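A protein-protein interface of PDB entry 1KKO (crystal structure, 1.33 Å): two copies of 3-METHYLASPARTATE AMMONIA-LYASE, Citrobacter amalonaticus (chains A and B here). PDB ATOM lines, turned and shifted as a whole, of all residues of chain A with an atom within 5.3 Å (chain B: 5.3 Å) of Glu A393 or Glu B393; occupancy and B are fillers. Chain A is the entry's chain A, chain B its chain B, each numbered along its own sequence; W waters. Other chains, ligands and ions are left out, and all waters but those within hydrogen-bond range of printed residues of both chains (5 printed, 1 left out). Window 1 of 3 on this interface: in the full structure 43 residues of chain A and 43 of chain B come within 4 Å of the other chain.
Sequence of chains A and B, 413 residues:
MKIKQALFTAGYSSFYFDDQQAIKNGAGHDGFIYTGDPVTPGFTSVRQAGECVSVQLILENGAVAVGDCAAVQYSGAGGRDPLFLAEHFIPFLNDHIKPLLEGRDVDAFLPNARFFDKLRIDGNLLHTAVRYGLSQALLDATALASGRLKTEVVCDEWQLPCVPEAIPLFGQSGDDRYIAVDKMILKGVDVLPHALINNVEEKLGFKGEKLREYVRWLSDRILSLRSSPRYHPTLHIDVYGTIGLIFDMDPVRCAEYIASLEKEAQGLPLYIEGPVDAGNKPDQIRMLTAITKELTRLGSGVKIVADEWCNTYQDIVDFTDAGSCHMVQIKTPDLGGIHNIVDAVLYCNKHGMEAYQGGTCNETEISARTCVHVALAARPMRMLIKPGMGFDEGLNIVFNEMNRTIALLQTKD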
ATOM      1  N   SER A  14       7.572  -8.720   3.855  1.00  0.00           N
ATOM      2  CA  SER A  14       6.689  -8.434   4.978  1.00  0.00           C
ATOM      3  C   SER A  14       7.194  -7.413   5.979  1.00  0.00           C
ATOM      4  O   SER A  14       6.626  -7.282   7.053  1.00  0.00           O
ATOM      5  CB  SER A  14       6.311  -9.721   5.690  1.00  0.00           C
ATOM      6  OG  SER A  14       5.373 -10.466   4.927  1.00  0.00           O
ATOM      7  N   PRO A 387       7.265 -14.323   8.449  1.00  0.00           N
ATOM      8  CA  PRO A 387       7.861 -13.001   8.547  1.00  0.00           C
ATOM      9  C   PRO A 387       6.902 -12.048   9.248  1.00  0.00           C
ATOM     10  O   PRO A 387       5.939 -12.483   9.874  1.00  0.00           O
ATOM     11  CB  PRO A 387       7.992 -12.626   7.077  1.00  0.00           C
ATOM     12  CG  PRO A 387       6.746 -13.171   6.491  1.00  0.00           C
ATOM     13  CD  PRO A 387       6.471 -14.454   7.226  1.00  0.00           C
ATOM     14  N   GLY A 388       7.190 -10.755   9.151  1.00  0.00           N
ATOM     15  CA  GLY A 388       6.321  -9.727   9.691  1.00  0.00           C
ATOM     16  C   GLY A 388       6.574  -9.347  11.125  1.00  0.00           C
ATOM     17  O   GLY A 388       7.207 -10.072  11.884  1.00  0.00           O
ATOM     18  N   MET A 389       6.045  -8.184  11.477  1.00  0.00           N
ATOM     19  CA  MET A 389       6.097  -7.673  12.839  1.00  0.00           C
ATOM     20  C   MET A 389       4.749  -7.755  13.536  1.00  0.00           C
ATOM     21  O   MET A 389       4.638  -7.379  14.694  1.00  0.00           O
ATOM     22  CB  MET A 389       6.657  -6.253  12.875  1.00  0.00           C
ATOM     23  CG  MET A 389       8.173  -6.232  12.704  1.00  0.00           C
ATOM     24  SD  MET A 389       9.081  -7.212  14.132  1.00  0.00           S
ATOM     25  CE  MET A 389      10.739  -6.326  14.176  1.00  0.00           C
ATOM     26  N   GLY A 390       3.725  -8.274  12.867  1.00  0.00           N
ATOM     27  CA  GLY A 390       2.427  -8.411  13.500  1.00  0.00           C
ATOM     28  C   GLY A 390       2.309  -9.615  14.408  1.00  0.00           C
ATOM     29  O   GLY A 390       1.380  -9.688  15.218  1.00  0.00           O
ATOM     30  N   PHE A 391       3.259 -10.543  14.269  1.00  0.00           N
ATOM     31  CA  PHE A 391       3.337 -11.815  14.991  1.00  0.00           C
ATOM     32  C   PHE A 391       2.246 -12.818  14.595  1.00  0.00           C
ATOM     33  O   PHE A 391       2.537 -13.972  14.273  1.00  0.00           O
ATOM     34  CB  PHE A 391       3.375 -11.645  16.521  1.00  0.00           C
ATOM     35  CG  PHE A 391       3.015 -12.905  17.241  1.00  0.00           C
ATOM     36  CD1 PHE A 391       1.755 -13.056  17.795  1.00  0.00           C
ATOM     37  CD2 PHE A 391       3.890 -13.987  17.285  1.00  0.00           C
ATOM     38  CE1 PHE A 391       1.389 -14.224  18.386  1.00  0.00           C
ATOM     39  CE2 PHE A 391       3.500 -15.162  17.888  1.00  0.00           C
ATOM     40  CZ  PHE A 391       2.252 -15.268  18.433  1.00  0.00           C
ATOM     41  N   ASP A 392       0.994 -12.391  14.605  1.00  0.00           N
ATOM     42  CA  ASP A 392      -0.103 -13.324  14.349  1.00  0.00           C
ATOM     43  C   ASP A 392       0.040 -14.000  13.003  1.00  0.00           C
ATOM     44  O   ASP A 392      -0.178 -15.212  12.859  1.00  0.00           O
ATOM     45  CB  ASP A 392      -1.443 -12.593  14.395  1.00  0.00           C
ATOM     46  CG  ASP A 392      -1.681 -11.911  15.686  1.00  0.00           C
ATOM     47  OD1 ASP A 392      -1.803 -12.623  16.715  1.00  0.00           O
ATOM     48  OD2 ASP A 392      -1.749 -10.656  15.747  1.00  0.00           O
ATOM     49  N   GLU A 393       0.373 -13.198  12.001  1.00  0.00           N
ATOM     50  CA  GLU A 393       0.493 -13.690  10.644  1.00  0.00           C
ATOM     51  C   GLU A 393       1.633 -14.690  10.524  1.00  0.00           C
ATOM     52  O   GLU A 393       1.476 -15.745   9.925  1.00  0.00           O
ATOM     53  CB  GLU A 393       0.689 -12.528   9.682  1.00  0.00           C
ATOM     54  CG  GLU A 393      -0.472 -11.538   9.649  1.00  0.00           C
ATOM     55  CD  GLU A 393      -0.324 -10.341  10.575  1.00  0.00           C
ATOM     56  OE1 GLU A 393      -0.718  -9.231  10.149  1.00  0.00           O
ATOM     57  OE2 GLU A 393       0.137 -10.493  11.725  1.00  0.00           O
ATOM     58  N   GLY A 394       2.789 -14.355  11.076  1.00  0.00           N
ATOM     59  CA  GLY A 394       3.919 -15.272  11.033  1.00  0.00           C
ATOM     60  C   GLY A 394       3.603 -16.567  11.752  1.00  0.00           C
ATOM     61  O   GLY A 394       4.034 -17.632  11.314  1.00  0.00           O
ATOM     62  N   LEU A 395       2.877 -16.509  12.859  1.00  0.00           N
ATOM     63  CA  LEU A 395       2.576 -17.740  13.571  1.00  0.00           C
ATOM     64  C   LEU A 395       1.653 -18.597  12.707  1.00  0.00           C
ATOM     65  O   LEU A 395       1.841 -19.806  12.576  1.00  0.00           O
ATOM     66  CB  LEU A 395       1.933 -17.466  14.933  1.00  0.00           C
ATOM     67  CG  LEU A 395       1.593 -18.746  15.704  1.00  0.00           C
ATOM     68  CD1 LEU A 395       2.853 -19.454  16.210  1.00  0.00           C
ATOM     69  CD2 LEU A 395       0.629 -18.436  16.846  1.00  0.00           C
ATOM     70  N   ASN A 396       0.635 -17.977  12.139  1.00  0.00           N
ATOM     71  CA  ASN A 396      -0.258 -18.678  11.231  1.00  0.00           C
ATOM     72  C   ASN A 396       0.563 -19.379  10.145  1.00  0.00           C
ATOM     73  O   ASN A 396       0.359 -20.548   9.858  1.00  0.00           O
ATOM     74  CB  ASN A 396      -1.212 -17.617  10.655  1.00  0.00           C
ATOM     75  CG  ASN A 396      -2.240 -18.155   9.699  1.00  0.00           C
ATOM     76  OD1 ASN A 396      -2.161 -19.288   9.182  1.00  0.00           O
ATOM     77  ND2 ASN A 396      -3.240 -17.322   9.446  1.00  0.00           N
ATOM     78  N   ILE A 397       1.493 -18.661   9.526  1.00  0.00           N
ATOM     79  CA  ILE A 397       2.302 -19.227   8.449  1.00  0.00           C
ATOM     80  C   ILE A 397       3.194 -20.383   8.923  1.00  0.00           C
ATOM     81  O   ILE A 397       3.200 -21.456   8.329  1.00  0.00           O
ATOM     82  CB  ILE A 397       3.142 -18.094   7.804  1.00  0.00           C
ATOM     83  CG1 ILE A 397       2.232 -17.171   6.972  1.00  0.00           C
ATOM     84  CG2 ILE A 397       4.296 -18.655   6.962  1.00  0.00           C
ATOM     85  CD1 ILE A 397       2.799 -15.813   6.750  1.00  0.00           C
ATOM     86  N   VAL A 398       3.950 -20.162   9.986  1.00  0.00           N
ATOM     87  CA  VAL A 398       4.944 -21.145  10.429  1.00  0.00           C
ATOM     88  C   VAL A 398       4.312 -22.321  11.180  1.00  0.00           C
ATOM     89  O   VAL A 398       4.541 -23.485  10.831  1.00  0.00           O
ATOM     90  CB  VAL A 398       6.025 -20.464  11.264  1.00  0.00           C
ATOM     91  CG1 VAL A 398       6.953 -21.485  11.859  1.00  0.00           C
ATOM     92  CG2 VAL A 398       6.812 -19.508  10.399  1.00  0.00           C
ATOM     93  N   SER B  14      -4.996 -15.567  11.752  1.00  0.00           N
ATOM     94  CA  SER B  14      -4.146 -14.395  11.892  1.00  0.00           C
ATOM     95  C   SER B  14      -4.668 -13.284  12.789  1.00  0.00           C
ATOM     96  O   SER B  14      -4.106 -12.193  12.797  1.00  0.00           O
ATOM     97  CB  SER B  14      -3.754 -13.846  10.518  1.00  0.00           C
ATOM     98  OG  SER B  14      -2.808 -14.704   9.882  1.00  0.00           O
ATOM     99  N   PRO B 387      -4.648 -11.895   5.507  1.00  0.00           N
ATOM    100  CA  PRO B 387      -5.266 -11.621   6.803  1.00  0.00           C
ATOM    101  C   PRO B 387      -4.350 -10.756   7.670  1.00  0.00           C
ATOM    102  O   PRO B 387      -3.385 -10.190   7.163  1.00  0.00           O
ATOM    103  CB  PRO B 387      -5.371 -13.009   7.393  1.00  0.00           C
ATOM    104  CG  PRO B 387      -4.103 -13.642   6.939  1.00  0.00           C
ATOM    105  CD  PRO B 387      -3.834 -13.119   5.551  1.00  0.00           C
ATOM    106  N   GLY B 388      -4.679 -10.657   8.952  1.00  0.00           N
ATOM    107  CA  GLY B 388      -3.873  -9.954   9.921  1.00  0.00           C
ATOM    108  C   GLY B 388      -4.098  -8.466  10.061  1.00  0.00           C
ATOM    109  O   GLY B 388      -4.675  -7.805   9.197  1.00  0.00           O
ATOM    110  N   MET B 389      -3.592  -7.939  11.167  1.00  0.00           N
ATOM    111  CA  MET B 389      -3.640  -6.517  11.451  1.00  0.00           C
ATOM    112  C   MET B 389      -2.274  -5.837  11.287  1.00  0.00           C
ATOM    113  O   MET B 389      -2.165  -4.627  11.472  1.00  0.00           O
ATOM    114  CB  MET B 389      -4.208  -6.264  12.846  1.00  0.00           C
ATOM    115  CG  MET B 389      -5.713  -6.477  12.903  1.00  0.00           C
ATOM    116  SD  MET B 389      -6.713  -5.367  11.624  1.00  0.00           S
ATOM    117  CE  MET B 389      -5.520  -3.934  11.538  1.00  0.00           C
ATOM    118  N   GLY B 390      -1.243  -6.582  10.897  1.00  0.00           N
ATOM    119  CA  GLY B 390       0.064  -5.981  10.663  1.00  0.00           C
ATOM    120  C   GLY B 390       0.203  -5.277   9.321  1.00  0.00           C
ATOM    121  O   GLY B 390       1.154  -4.509   9.124  1.00  0.00           O
ATOM    122  N   PHE B 391      -0.737  -5.548   8.414  1.00  0.00           N
ATOM    123  CA  PHE B 391      -0.780  -5.020   7.055  1.00  0.00           C
ATOM    124  C   PHE B 391       0.322  -5.569   6.129  1.00  0.00           C
ATOM    125  O   PHE B 391       0.038  -6.079   5.032  1.00  0.00           O
ATOM    126  CB  PHE B 391      -0.819  -3.470   6.999  1.00  0.00           C
ATOM    127  CG  PHE B 391      -0.457  -2.944   5.641  1.00  0.00           C
ATOM    128  CD1 PHE B 391       0.799  -2.436   5.411  1.00  0.00           C
ATOM    129  CD2 PHE B 391      -1.328  -3.065   4.568  1.00  0.00           C
ATOM    130  CE1 PHE B 391       1.180  -2.045   4.162  1.00  0.00           C
ATOM    131  CE2 PHE B 391      -0.934  -2.652   3.309  1.00  0.00           C
ATOM    132  CZ  PHE B 391       0.325  -2.140   3.135  1.00  0.00           C
ATOM    133  N   ASP B 392       1.579  -5.483   6.560  1.00  0.00           N
ATOM    134  CA  ASP B 392       2.679  -5.871   5.695  1.00  0.00           C
ATOM    135  C   ASP B 392       2.524  -7.299   5.217  1.00  0.00           C
ATOM    136  O   ASP B 392       2.757  -7.612   4.048  1.00  0.00           O
ATOM    137  CB  ASP B 392       4.000  -5.720   6.430  1.00  0.00           C
ATOM    138  CG  ASP B 392       4.226  -4.342   6.904  1.00  0.00           C
ATOM    139  OD1 ASP B 392       4.333  -3.439   6.044  1.00  0.00           O
ATOM    140  OD2 ASP B 392       4.289  -4.098   8.129  1.00  0.00           O
ATOM    141  N   GLU B 393       2.212  -8.178   6.155  1.00  0.00           N
ATOM    142  CA  GLU B 393       2.122  -9.595   5.866  1.00  0.00           C
ATOM    143  C   GLU B 393       0.995  -9.875   4.885  1.00  0.00           C
ATOM    144  O   GLU B 393       1.162 -10.620   3.927  1.00  0.00           O
ATOM    145  CB  GLU B 393       1.904 -10.365   7.157  1.00  0.00           C
ATOM    146  CG  GLU B 393       3.035 -10.208   8.160  1.00  0.00           C
ATOM    147  CD  GLU B 393       2.830  -9.133   9.210  1.00  0.00           C
ATOM    148  OE1 GLU B 393       3.193  -9.379  10.383  1.00  0.00           O
ATOM    149  OE2 GLU B 393       2.350  -8.036   8.855  1.00  0.00           O
ATOM    150  N   GLY B 394      -0.166  -9.272   5.114  1.00  0.00           N
ATOM    151  CA  GLY B 394      -1.286  -9.435   4.205  1.00  0.00           C
ATOM    152  C   GLY B 394      -0.979  -8.928   2.812  1.00  0.00           C
ATOM    153  O   GLY B 394      -1.371  -9.550   1.841  1.00  0.00           O
ATOM    154  N   LEU B 395      -0.259  -7.820   2.716  1.00  0.00           N
ATOM    155  CA  LEU B 395       0.069  -7.295   1.397  1.00  0.00           C
ATOM    156  C   LEU B 395       0.985  -8.265   0.675  1.00  0.00           C
ATOM    157  O   LEU B 395       0.789  -8.573  -0.500  1.00  0.00           O
ATOM    158  CB  LEU B 395       0.709  -5.912   1.464  1.00  0.00           C
ATOM    159  CG  LEU B 395       1.072  -5.333   0.098  1.00  0.00           C
ATOM    160  CD1 LEU B 395      -0.149  -4.935  -0.702  1.00  0.00           C
ATOM    161  CD2 LEU B 395       1.990  -4.147   0.272  1.00  0.00           C
ATOM    162  N   ASN B 396       1.997  -8.747   1.379  1.00  0.00           N
ATOM    163  CA  ASN B 396       2.897  -9.739   0.816  1.00  0.00           C
ATOM    164  C   ASN B 396       2.100 -10.939   0.266  1.00  0.00           C
ATOM    165  O   ASN B 396       2.317 -11.384  -0.865  1.00  0.00           O
ATOM    166  CB  ASN B 396       3.865 -10.136   1.929  1.00  0.00           C
ATOM    167  CG  ASN B 396       4.889 -11.154   1.535  1.00  0.00           C
ATOM    168  OD1 ASN B 396       4.802 -11.849   0.501  1.00  0.00           O
ATOM    169  ND2 ASN B 396       5.890 -11.257   2.396  1.00  0.00           N
ATOM    170  N   ILE B 397       1.161 -11.438   1.056  1.00  0.00           N
ATOM    171  CA  ILE B 397       0.369 -12.579   0.659  1.00  0.00           C
ATOM    172  C   ILE B 397      -0.501 -12.296  -0.551  1.00  0.00           C
ATOM    173  O   ILE B 397      -0.497 -13.054  -1.523  1.00  0.00           O
ATOM    174  CB  ILE B 397      -0.477 -13.047   1.859  1.00  0.00           C
ATOM    175  CG1 ILE B 397       0.408 -13.718   2.911  1.00  0.00           C
ATOM    176  CG2 ILE B 397      -1.598 -13.988   1.431  1.00  0.00           C
ATOM    177  CD1 ILE B 397      -0.179 -13.764   4.278  1.00  0.00           C
ATOM    178  N   VAL B 398      -1.253 -11.203  -0.508  1.00  0.00           N
ATOM    179  CA  VAL B 398      -2.241 -10.941  -1.544  1.00  0.00           C
ATOM    180  C   VAL B 398      -1.614 -10.364  -2.806  1.00  0.00           C
ATOM    181  O   VAL B 398      -1.840 -10.870  -3.909  1.00  0.00           O
ATOM    182  CB  VAL B 398      -3.354 -10.019  -1.004  1.00  0.00           C
ATOM    183  CG1 VAL B 398      -4.293  -9.557  -2.108  1.00  0.00           C
ATOM    184  CG2 VAL B 398      -4.132 -10.729   0.087  1.00  0.00           C
HETATM  185  O   HOH W   1      -1.329  -8.303   7.622  1.00  0.00           O
HETATM  186  O   HOH W   2       4.185  -6.253  10.028  1.00  0.00           O
HETATM  187  O   HOH W   3       3.419 -12.586   4.650  1.00  0.00           O
HETATM  188  O   HOH W   4      -0.747 -15.376   7.784  1.00  0.00           O
HETATM  189  O   HOH W   5       3.895 -11.729  11.660  1.00  0.00           O
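The side-chain carboxylate (OE1) of Glu A393 is in hydrogen-bond range of the backbone NH (N) of Met B389 (3.3 Å). The side-chain carboxylate (OE1) of Glu A393 lies within hydrogen-bond range of the backbone NH (N) of Gly B390 (2.8 Å). The side-chain carboxylate of Glu B393 lies within hydrogen-bond range of the backbone NH of Gly A390, 2.8 Å away. ND2 of Asn A396 sits at hydrogen-bond distance from OG of Ser B14 (2.7 Å). The side-chain hydroxyl of Ser A14 is in hydrogen-bond range of the side-chain amide nitrogen of Asn B396 (2.7 Å). The side-chain carboxylate (OE1) of Glu B393 is in hydrogen-bond range of the backbone NH (N) of Met A389 (3.3 Å).
Among the printed residues, pairs that only touch across the chains: Ser A14 with Asp B392 (3.1 Å), Asp A392 with Ser B14 (3.1 Å), Gly A388 with Glu B393 (3.2 Å), Glu A393 with Gly B388 (3.2 Å), Ser A14 with Glu B393 (3.5 Å), Glu A393 with Glu B393 (3.5 Å) and Glu A393 with Ser B14 (3.5 Å).
Of the printed residues of chain B, Gly A388 touches Glu B393. Of the printed residues of chain B, Gly A390 touches Glu B393 (2.8 Å). Leu A395 touches none of the printed residues of chain B. Printed residues of chain B within 4 Å of Asn A396: Ser B14 (2.7 Å). Of the printed residues of chain A, Glu B393 touches Ser A14, Gly A388, Met A389, Gly A390 and Glu A393. Val B398 touches none of the printed residues of chain A.
Of the 13 printed residues of chain B, 7 touch a printed residue of chain A.
Gly A388 touches Glu B393, and with the chains exchanged Glu A393 touches Gly B388. Met A389 touches Glu B393, and with the chains exchanged Glu A393 touches Met B389. Gly A390 touches Glu B393, and with the chains exchanged Glu A393 touches Gly B390. Glu B393 touches its own counterpart, Glu A393. Positions printed for both chains: 14, 387, 388, 389, 390, 391, 392, 393, 394, 395, 396, 397 and 398. Of the 13 pairs that touch across the chains among the printed residues, 13 have their exchanged pair printed and touching as well.
Water W1 lies within hydrogen-bond range of the side-chain carboxylate (OE1) of Glu A393, the backbone carbonyl oxygen (O) of Pro B387, the backbone NH (N) of Phe B391 and the backbone NH (N) of Gly B394. Water W5 lies within hydrogen-bond range of the side-chain carboxylate (OE1) of Glu B393 (2.8 Å), the backbone carbonyl oxygen (O) of Pro A387 (2.8 Å), the backbone NH (N) of Gly A394 (2.9 Å) and the backbone NH (N) of Phe A391 (2.9 Å). Water W2 lies within hydrogen-bond range of OE2 of Glu B393, OD2 of Asp B392 and N of Met A389. Water W3 lies within hydrogen-bond range of the side-chain hydroxyl (OG) of Ser A14 and the backbone carbonyl oxygen (O) of Glu B393. Water W4 lies within hydrogen-bond range of the side-chain hydroxyl (OG) of Ser B14 and the backbone carbonyl oxygen (O) of Glu A393.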
